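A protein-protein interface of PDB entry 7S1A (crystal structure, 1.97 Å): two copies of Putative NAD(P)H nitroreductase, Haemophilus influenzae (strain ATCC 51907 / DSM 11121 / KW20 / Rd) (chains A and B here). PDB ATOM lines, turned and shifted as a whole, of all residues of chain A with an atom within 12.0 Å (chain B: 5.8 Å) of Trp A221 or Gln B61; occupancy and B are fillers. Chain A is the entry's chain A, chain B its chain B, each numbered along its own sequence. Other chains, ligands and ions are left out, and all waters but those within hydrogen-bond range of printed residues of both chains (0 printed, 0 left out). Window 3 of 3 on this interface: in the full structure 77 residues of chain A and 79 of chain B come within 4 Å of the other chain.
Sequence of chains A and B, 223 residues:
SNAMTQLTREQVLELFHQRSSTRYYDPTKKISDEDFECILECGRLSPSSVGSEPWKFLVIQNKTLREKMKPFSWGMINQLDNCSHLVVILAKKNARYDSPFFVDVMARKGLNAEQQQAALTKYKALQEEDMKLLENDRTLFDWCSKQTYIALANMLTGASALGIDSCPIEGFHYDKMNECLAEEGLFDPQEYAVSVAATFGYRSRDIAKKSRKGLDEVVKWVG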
ATOM      1  N   GLY A 214      -8.108  15.928   4.110  1.00  0.00           N
ATOM      2  CA  GLY A 214      -9.055  16.631   3.272  1.00  0.00           C
ATOM      3  C   GLY A 214     -10.126  15.701   2.740  1.00  0.00           C
ATOM      4  O   GLY A 214      -9.922  14.497   2.596  1.00  0.00           O
ATOM      5  N   LEU A 215     -11.297  16.276   2.448  1.00  0.00           N
ATOM      6  CA  LEU A 215     -12.372  15.466   1.893  1.00  0.00           C
ATOM      7  C   LEU A 215     -11.996  14.925   0.521  1.00  0.00           C
ATOM      8  O   LEU A 215     -12.374  13.802   0.173  1.00  0.00           O
ATOM      9  CB  LEU A 215     -13.662  16.276   1.827  1.00  0.00           C
ATOM     10  CG  LEU A 215     -14.948  15.460   1.688  1.00  0.00           C
ATOM     11  CD1 LEU A 215     -15.121  14.461   2.833  1.00  0.00           C
ATOM     12  CD2 LEU A 215     -16.147  16.395   1.581  1.00  0.00           C
ATOM     13  N   ASP A 216     -11.218  15.694  -0.247  1.00  0.00           N
ATOM     14  CA  ASP A 216     -10.745  15.247  -1.552  1.00  0.00           C
ATOM     15  C   ASP A 216      -9.761  14.081  -1.448  1.00  0.00           C
ATOM     16  O   ASP A 216      -9.626  13.303  -2.400  1.00  0.00           O
ATOM     17  CB  ASP A 216     -10.101  16.421  -2.290  1.00  0.00           C
ATOM     18  CG  ASP A 216     -11.101  17.495  -2.656  1.00  0.00           C
ATOM     19  OD1 ASP A 216     -12.240  17.141  -3.030  1.00  0.00           O
ATOM     20  OD2 ASP A 216     -10.748  18.692  -2.566  1.00  0.00           O
ATOM     21  N   GLU A 217      -9.053  13.951  -0.324  1.00  0.00           N
ATOM     22  CA  GLU A 217      -8.142  12.820  -0.146  1.00  0.00           C
ATOM     23  C   GLU A 217      -8.871  11.553   0.287  1.00  0.00           C
ATOM     24  O   GLU A 217      -8.484  10.449  -0.115  1.00  0.00           O
ATOM     25  CB  GLU A 217      -7.054  13.179   0.873  1.00  0.00           C
ATOM     26  CG  GLU A 217      -6.043  14.191   0.347  1.00  0.00           C
ATOM     27  CD  GLU A 217      -5.135  14.767   1.425  1.00  0.00           C
ATOM     28  OE1 GLU A 217      -5.520  14.760   2.610  1.00  0.00           O
ATOM     29  OE2 GLU A 217      -4.027  15.235   1.077  1.00  0.00           O
ATOM     30  N   VAL A 218      -9.935  11.685   1.078  1.00  0.00           N
ATOM     31  CA  VAL A 218     -10.568  10.517   1.671  1.00  0.00           C
ATOM     32  C   VAL A 218     -11.754   9.987   0.857  1.00  0.00           C
ATOM     33  O   VAL A 218     -12.117   8.810   0.999  1.00  0.00           O
ATOM     34  CB  VAL A 218     -10.950  10.861   3.124  1.00  0.00           C
ATOM     35  CG1 VAL A 218     -12.076  11.882   3.188  1.00  0.00           C
ATOM     36  CG2 VAL A 218     -11.297   9.618   3.885  1.00  0.00           C
ATOM     37  N   VAL A 219     -12.343  10.797  -0.014  1.00  0.00           N
ATOM     38  CA  VAL A 219     -13.483  10.392  -0.834  1.00  0.00           C
ATOM     39  C   VAL A 219     -12.998  10.130  -2.253  1.00  0.00           C
ATOM     40  O   VAL A 219     -12.279  10.957  -2.828  1.00  0.00           O
ATOM     41  CB  VAL A 219     -14.569  11.483  -0.833  1.00  0.00           C
ATOM     42  CG1 VAL A 219     -15.683  11.134  -1.814  1.00  0.00           C
ATOM     43  CG2 VAL A 219     -15.109  11.683   0.556  1.00  0.00           C
ATOM     44  N   LYS A 220     -13.388   8.986  -2.824  1.00  0.00           N
ATOM     45  CA  LYS A 220     -13.215   8.712  -4.251  1.00  0.00           C
ATOM     46  C   LYS A 220     -14.590   8.480  -4.882  1.00  0.00           C
ATOM     47  O   LYS A 220     -15.339   7.595  -4.449  1.00  0.00           O
ATOM     48  CB  LYS A 220     -12.301   7.505  -4.496  1.00  0.00           C
ATOM     49  CG  LYS A 220     -12.167   7.135  -6.001  1.00  0.00           C
ATOM     50  CD  LYS A 220     -10.719   6.836  -6.386  1.00  0.00           C
ATOM     51  CE  LYS A 220     -10.566   6.522  -7.870  1.00  0.00           C
ATOM     52  NZ  LYS A 220     -10.531   7.746  -8.729  1.00  0.00           N
ATOM     53  N   TRP A 221     -14.926   9.270  -5.897  1.00  0.00           N
ATOM     54  CA  TRP A 221     -16.252   9.238  -6.497  1.00  0.00           C
ATOM     55  C   TRP A 221     -16.236   8.383  -7.761  1.00  0.00           C
ATOM     56  O   TRP A 221     -15.375   8.568  -8.628  1.00  0.00           O
ATOM     57  CB  TRP A 221     -16.732  10.652  -6.825  1.00  0.00           C
ATOM     58  CG  TRP A 221     -18.213  10.735  -6.863  1.00  0.00           C
ATOM     59  CD1 TRP A 221     -19.032  10.370  -7.901  1.00  0.00           C
ATOM     60  CD2 TRP A 221     -19.078  11.189  -5.809  1.00  0.00           C
ATOM     61  NE1 TRP A 221     -20.352  10.576  -7.554  1.00  0.00           N
ATOM     62  CE2 TRP A 221     -20.405  11.081  -6.279  1.00  0.00           C
ATOM     63  CE3 TRP A 221     -18.858  11.689  -4.524  1.00  0.00           C
ATOM     64  CZ2 TRP A 221     -21.507  11.443  -5.503  1.00  0.00           C
ATOM     65  CZ3 TRP A 221     -19.959  12.057  -3.754  1.00  0.00           C
ATOM     66  CH2 TRP A 221     -21.265  11.935  -4.251  1.00  0.00           C
ATOM     67  N   VAL A 222     -17.194   7.459  -7.862  1.00  0.00           N
ATOM     68  CA  VAL A 222     -17.309   6.527  -8.993  1.00  0.00           C
ATOM     69  C   VAL A 222     -18.681   6.751  -9.619  1.00  0.00           C
ATOM     70  O   VAL A 222     -19.669   6.133  -9.214  1.00  0.00           O
ATOM     71  CB  VAL A 222     -17.143   5.067  -8.562  1.00  0.00           C
ATOM     72  CG1 VAL A 222     -16.958   4.171  -9.782  1.00  0.00           C
ATOM     73  CG2 VAL A 222     -15.979   4.909  -7.560  1.00  0.00           C
ATOM     74  N   GLY A 223     -18.762   7.620 -10.618  1.00  0.00           N
ATOM     75  CA  GLY A 223     -20.053   7.980 -11.193  1.00  0.00           C
ATOM     76  C   GLY A 223     -20.282   7.417 -12.586  1.00  0.00           C
ATOM     77  O   GLY A 223     -19.493   6.582 -13.043  1.00  0.00           O
ATOM     78  N   ASP B  33     -26.655  16.550  -3.712  1.00  0.00           N
ATOM     79  CA  ASP B  33     -25.206  16.591  -3.526  1.00  0.00           C
ATOM     80  C   ASP B  33     -24.838  17.206  -2.179  1.00  0.00           C
ATOM     81  O   ASP B  33     -23.968  16.689  -1.460  1.00  0.00           O
ATOM     82  CB  ASP B  33     -24.556  17.369  -4.676  1.00  0.00           C
ATOM     83  CG  ASP B  33     -24.746  16.684  -6.035  1.00  0.00           C
ATOM     84  OD1 ASP B  33     -24.880  15.446  -6.058  1.00  0.00           O
ATOM     85  OD2 ASP B  33     -24.760  17.372  -7.080  1.00  0.00           O
ATOM     86  N   PHE B  36     -25.504  14.812   0.630  1.00  0.00           N
ATOM     87  CA  PHE B  36     -24.620  13.670   0.715  1.00  0.00           C
ATOM     88  C   PHE B  36     -23.224  14.075   1.156  1.00  0.00           C
ATOM     89  O   PHE B  36     -22.573  13.320   1.886  1.00  0.00           O
ATOM     90  CB  PHE B  36     -24.547  12.905  -0.594  1.00  0.00           C
ATOM     91  CG  PHE B  36     -23.889  11.588  -0.418  1.00  0.00           C
ATOM     92  CD1 PHE B  36     -24.490  10.624   0.373  1.00  0.00           C
ATOM     93  CD2 PHE B  36     -22.647  11.333  -0.955  1.00  0.00           C
ATOM     94  CE1 PHE B  36     -23.895   9.417   0.583  1.00  0.00           C
ATOM     95  CE2 PHE B  36     -22.040  10.118  -0.736  1.00  0.00           C
ATOM     96  CZ  PHE B  36     -22.671   9.162   0.026  1.00  0.00           C
ATOM     97  N   LEU B  40     -20.930  12.497   4.175  1.00  0.00           N
ATOM     98  CA  LEU B  40     -19.515  12.146   4.078  1.00  0.00           C
ATOM     99  C   LEU B  40     -18.687  12.914   5.097  1.00  0.00           C
ATOM    100  O   LEU B  40     -17.753  12.365   5.702  1.00  0.00           O
ATOM    101  CB  LEU B  40     -19.001  12.420   2.672  1.00  0.00           C
ATOM    102  CG  LEU B  40     -19.568  11.530   1.566  1.00  0.00           C
ATOM    103  CD1 LEU B  40     -19.212  12.156   0.234  1.00  0.00           C
ATOM    104  CD2 LEU B  40     -19.004  10.145   1.677  1.00  0.00           C
ATOM    105  N   PHE B  57     -13.481   6.430   1.303  1.00  0.00           N
ATOM    106  CA  PHE B  57     -14.905   6.272   1.026  1.00  0.00           C
ATOM    107  C   PHE B  57     -15.125   6.240  -0.486  1.00  0.00           C
ATOM    108  O   PHE B  57     -15.049   7.271  -1.156  1.00  0.00           O
ATOM    109  CB  PHE B  57     -15.697   7.401   1.674  1.00  0.00           C
ATOM    110  CG  PHE B  57     -15.367   7.623   3.117  1.00  0.00           C
ATOM    111  CD1 PHE B  57     -15.707   6.681   4.074  1.00  0.00           C
ATOM    112  CD2 PHE B  57     -14.758   8.796   3.530  1.00  0.00           C
ATOM    113  CE1 PHE B  57     -15.425   6.888   5.404  1.00  0.00           C
ATOM    114  CE2 PHE B  57     -14.472   9.008   4.866  1.00  0.00           C
ATOM    115  CZ  PHE B  57     -14.795   8.049   5.805  1.00  0.00           C
ATOM    116  N   LEU B  58     -15.387   5.052  -1.027  1.00  0.00           N
ATOM    117  CA  LEU B  58     -15.739   4.909  -2.434  1.00  0.00           C
ATOM    118  C   LEU B  58     -17.242   5.099  -2.574  1.00  0.00           C
ATOM    119  O   LEU B  58     -18.017   4.299  -2.031  1.00  0.00           O
ATOM    120  CB  LEU B  58     -15.349   3.533  -2.967  1.00  0.00           C
ATOM    121  CG  LEU B  58     -13.907   3.050  -2.952  1.00  0.00           C
ATOM    122  CD1 LEU B  58     -13.810   1.735  -3.729  1.00  0.00           C
ATOM    123  CD2 LEU B  58     -12.985   4.073  -3.542  1.00  0.00           C
ATOM    124  N   VAL B  59     -17.660   6.130  -3.309  1.00  0.00           N
ATOM    125  CA  VAL B  59     -19.075   6.355  -3.613  1.00  0.00           C
ATOM    126  C   VAL B  59     -19.378   5.716  -4.972  1.00  0.00           C
ATOM    127  O   VAL B  59     -18.919   6.195  -6.017  1.00  0.00           O
ATOM    128  CB  VAL B  59     -19.429   7.849  -3.599  1.00  0.00           C
ATOM    129  CG1 VAL B  59     -20.926   8.030  -3.659  1.00  0.00           C
ATOM    130  CG2 VAL B  59     -18.850   8.536  -2.346  1.00  0.00           C
ATOM    131  N   ILE B  60     -20.172   4.645  -4.979  1.00  0.00           N
ATOM    132  CA  ILE B  60     -20.387   3.845  -6.190  1.00  0.00           C
ATOM    133  C   ILE B  60     -21.742   4.244  -6.769  1.00  0.00           C
ATOM    134  O   ILE B  60     -22.780   3.659  -6.448  1.00  0.00           O
ATOM    135  CB  ILE B  60     -20.308   2.348  -5.910  1.00  0.00           C
ATOM    136  CG1 ILE B  60     -19.054   2.008  -5.075  1.00  0.00           C
ATOM    137  CG2 ILE B  60     -20.345   1.567  -7.237  1.00  0.00           C
ATOM    138  CD1 ILE B  60     -17.735   2.179  -5.826  1.00  0.00           C
ATOM    139  N   GLN B  61     -21.736   5.232  -7.656  1.00  0.00           N
ATOM    140  CA  GLN B  61     -22.958   5.658  -8.317  1.00  0.00           C
ATOM    141  C   GLN B  61     -23.144   5.019  -9.690  1.00  0.00           C
ATOM    142  O   GLN B  61     -24.280   4.907 -10.164  1.00  0.00           O
ATOM    143  CB  GLN B  61     -22.976   7.188  -8.441  1.00  0.00           C
ATOM    144  CG  GLN B  61     -22.841   7.898  -7.101  1.00  0.00           C
ATOM    145  CD  GLN B  61     -23.939   7.484  -6.137  1.00  0.00           C
ATOM    146  OE1 GLN B  61     -23.776   6.548  -5.370  1.00  0.00           O
ATOM    147  NE2 GLN B  61     -25.089   8.154  -6.219  1.00  0.00           N
ATOM    148  N   ASN B  62     -22.056   4.609 -10.330  1.00  0.00           N
ATOM    149  CA  ASN B  62     -22.076   3.972 -11.647  1.00  0.00           C
ATOM    150  C   ASN B  62     -23.025   2.780 -11.672  1.00  0.00           C
ATOM    151  O   ASN B  62     -22.821   1.804 -10.952  1.00  0.00           O
ATOM    152  CB  ASN B  62     -20.647   3.529 -11.985  1.00  0.00           C
ATOM    153  CG  ASN B  62     -20.524   2.916 -13.349  1.00  0.00           C
ATOM    154  OD1 ASN B  62     -20.823   1.743 -13.544  1.00  0.00           O
ATOM    155  ND2 ASN B  62     -20.043   3.695 -14.301  1.00  0.00           N
ATOM    156  N   LYS B  63     -24.074   2.860 -12.495  1.00  0.00           N
ATOM    157  CA  LYS B  63     -25.050   1.776 -12.509  1.00  0.00           C
ATOM    158  C   LYS B  63     -24.388   0.465 -12.904  1.00  0.00           C
ATOM    159  O   LYS B  63     -24.590  -0.566 -12.253  1.00  0.00           O
ATOM    160  CB  LYS B  63     -26.207   2.103 -13.452  1.00  0.00           C
ATOM    161  CG  LYS B  63     -27.148   3.236 -12.973  1.00  0.00           C
ATOM    162  CD  LYS B  63     -27.412   3.181 -11.458  1.00  0.00           C
ATOM    163  CE  LYS B  63     -28.374   2.055 -11.052  1.00  0.00           C
ATOM    164  NZ  LYS B  63     -28.267   1.691  -9.601  1.00  0.00           N
ATOM    165  N   ARG B  66     -22.514  -1.099 -10.051  1.00  0.00           N
ATOM    166  CA  ARG B  66     -23.486  -1.636  -9.101  1.00  0.00           C
ATOM    167  C   ARG B  66     -24.039  -2.973  -9.587  1.00  0.00           C
ATOM    168  O   ARG B  66     -24.119  -3.943  -8.825  1.00  0.00           O
ATOM    169  CB  ARG B  66     -24.619  -0.641  -8.892  1.00  0.00           C
ATOM    170  CG  ARG B  66     -24.317   0.450  -7.883  1.00  0.00           C
ATOM    171  CD  ARG B  66     -25.541   1.363  -7.770  1.00  0.00           C
ATOM    172  NE  ARG B  66     -25.233   2.556  -6.995  1.00  0.00           N
ATOM    173  CZ  ARG B  66     -26.140   3.349  -6.451  1.00  0.00           C
ATOM    174  NH1 ARG B  66     -27.431   3.124  -6.603  1.00  0.00           N
ATOM    175  NH2 ARG B  66     -25.738   4.371  -5.707  1.00  0.00           N
ATOM    176  N   SER B  84     -30.218   5.665  -3.424  1.00  0.00           N
ATOM    177  CA  SER B  84     -29.639   6.902  -3.955  1.00  0.00           C
ATOM    178  C   SER B  84     -28.131   6.784  -4.104  1.00  0.00           C
ATOM    179  O   SER B  84     -27.588   6.982  -5.198  1.00  0.00           O
ATOM    180  CB  SER B  84     -29.986   8.082  -3.046  1.00  0.00           C
ATOM    181  OG  SER B  84     -29.563   9.325  -3.602  1.00  0.00           O
ATOM    182  N   HIS B  85     -27.441   6.436  -3.012  1.00  0.00           N
ATOM    183  CA  HIS B  85     -25.988   6.429  -2.951  1.00  0.00           C
ATOM    184  C   HIS B  85     -25.505   5.161  -2.263  1.00  0.00           C
ATOM    185  O   HIS B  85     -26.165   4.641  -1.364  1.00  0.00           O
ATOM    186  CB  HIS B  85     -25.431   7.611  -2.157  1.00  0.00           C
ATOM    187  CG  HIS B  85     -25.520   8.921  -2.860  1.00  0.00           C
ATOM    188  ND1 HIS B  85     -26.714   9.569  -3.070  1.00  0.00           N
ATOM    189  CD2 HIS B  85     -24.558   9.720  -3.376  1.00  0.00           C
ATOM    190  CE1 HIS B  85     -26.487  10.709  -3.702  1.00  0.00           C
ATOM    191  NE2 HIS B  85     -25.185  10.824  -3.899  1.00  0.00           N
ATOM    192  N   LEU B  86     -24.330   4.698  -2.666  1.00  0.00           N
ATOM    193  CA  LEU B  86     -23.660   3.563  -2.040  1.00  0.00           C
ATOM    194  C   LEU B  86     -22.247   3.989  -1.699  1.00  0.00           C
ATOM    195  O   LEU B  86     -21.572   4.607  -2.533  1.00  0.00           O
ATOM    196  CB  LEU B  86     -23.642   2.342  -2.977  1.00  0.00           C
ATOM    197  CG  LEU B  86     -22.590   1.229  -2.802  1.00  0.00           C
ATOM    198  CD1 LEU B  86     -22.869   0.362  -1.602  1.00  0.00           C
ATOM    199  CD2 LEU B  86     -22.544   0.358  -4.052  1.00  0.00           C
ATOM    200  N   LEU B 186      -9.850   1.250  -8.782  1.00  0.00           N
ATOM    201  CA  LEU B 186     -10.412   2.191  -7.829  1.00  0.00           C
ATOM    202  C   LEU B 186      -9.600   2.306  -6.544  1.00  0.00           C
ATOM    203  O   LEU B 186      -9.838   3.239  -5.772  1.00  0.00           O
ATOM    204  CB  LEU B 186     -11.858   1.807  -7.508  1.00  0.00           C
ATOM    205  CG  LEU B 186     -12.838   2.050  -8.655  1.00  0.00           C
ATOM    206  CD1 LEU B 186     -14.195   1.515  -8.280  1.00  0.00           C
ATOM    207  CD2 LEU B 186     -12.927   3.527  -9.000  1.00  0.00           C
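Of the 10 printed residues of chain A, 6 touch a printed residue of chain B.
Hydrophobic or aromatic side chains of chain A within 4 Å of the printed part of chain B: Val A218, Val A219, Trp A221 and Val A222.
Among the printed residues, 15 pairs touch across the chains.
Among the printed residues, no Asp or Glu carboxylate lies within 4 Å of a Lys or Arg side-chain nitrogen of the other chain.
The backbone carbonyl oxygen of Ile B60 lies within hydrogen-bond range of the guanidinium group of Arg B66 (2.7 Å).
N of Ile B60 sits at hydrogen-bond distance from O of Leu B86 (2.8 Å).
The side-chain amide oxygen of Gln B61 is in hydrogen-bond range of the guanidinium group of Arg B66 (2.9 Å).
The side-chain amide nitrogen (NE2) of Gln B61 sits at hydrogen-bond distance from the backbone carbonyl oxygen (O) of Ser B84 (2.9 Å).
The side-chain amide oxygen (OE1) of Gln B61 sits at hydrogen-bond distance from the backbone NH (N) of Leu B86 (3.3 Å).
No position is printed for both chains.
Of the 15 pairs that touch across the chains among the printed residues, none has its exchanged pair printed and touching as well.
Val A219 touches Phe B57.
Leu B58 touches Lys A220 (CA to O, 3.4 Å).
Lys A220 touches Leu B186.
Trp A221 touches Phe B36.
Val B59 touches Trp A221.
Gln B61 touches Trp A221.
CG2 of Val A222 touches CD1 of Ile B60 (3.7 Å).
Leu B186 touches Val A222.
The backbone carbonyl oxygen of Val A218 lies within hydrogen-bond range of the backbone NH of Phe B57 (2.8 Å).
O of Phe B57 is in hydrogen-bond range of N of Lys A220 (2.9 Å).
O of Lys A220 lies within hydrogen-bond range of N of Val B59, 3.0 Å away.
The backbone NH (N) of Val A222 sits at hydrogen-bond distance from the backbone carbonyl oxygen (O) of Val B59, 2.8 Å away.
The backbone carbonyl oxygen (O) of Val A222 sits at hydrogen-bond distance from the backbone NH (N) of Gln B61 (2.7 Å).
The backbone carbonyl oxygen (O) of Val A222 lies within hydrogen-bond range of the backbone NH (N) of Asn B62.
The backbone carbonyl oxygen (O) of Gly A223 lies within hydrogen-bond range of the side-chain amide nitrogen (ND2) of Asn B62, 3.2 Å away.
Gln B61 touches just these residues of chain A: Trp A221 (3.7 Å) and Val A222 (2.7 Å).
Of chain A, only Trp A221 comes within 4 Å of Phe B36.
Val B59 touches three residues of chain A.
Asn B62 touches just these residues of chain A: Val A222 (3.0 Å) and Gly A223 (3.2 Å).
No residue of chain A comes within 4 Å of Ser B84.
No residue of chain A comes within 4 Å of His B85.
Printed residues of chain A within 4 Å of Leu B186: Lys A220 and Val A222.
Printed residues of chain B within 4 Å of Val A222: Val B59 (2.8 Å), Ile B60 (3.7 Å), Gln B61 (2.7 Å), Asn B62 (3.0 Å) and Leu B186 (3.6 Å).
Of the printed residues of chain B, Val A218 touches Phe B57.
Printed residues of chain B within 4 Å of Gly A223: Asn B62.
Asp A216 touches none of the printed residues of chain B.
The nearest printed residue of chain B that does not touch Trp A221 is Leu B40 (4.1 Å).
The nearest residue of chain A that does not touch Gln B61 is Gly A223 (4.1 Å).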
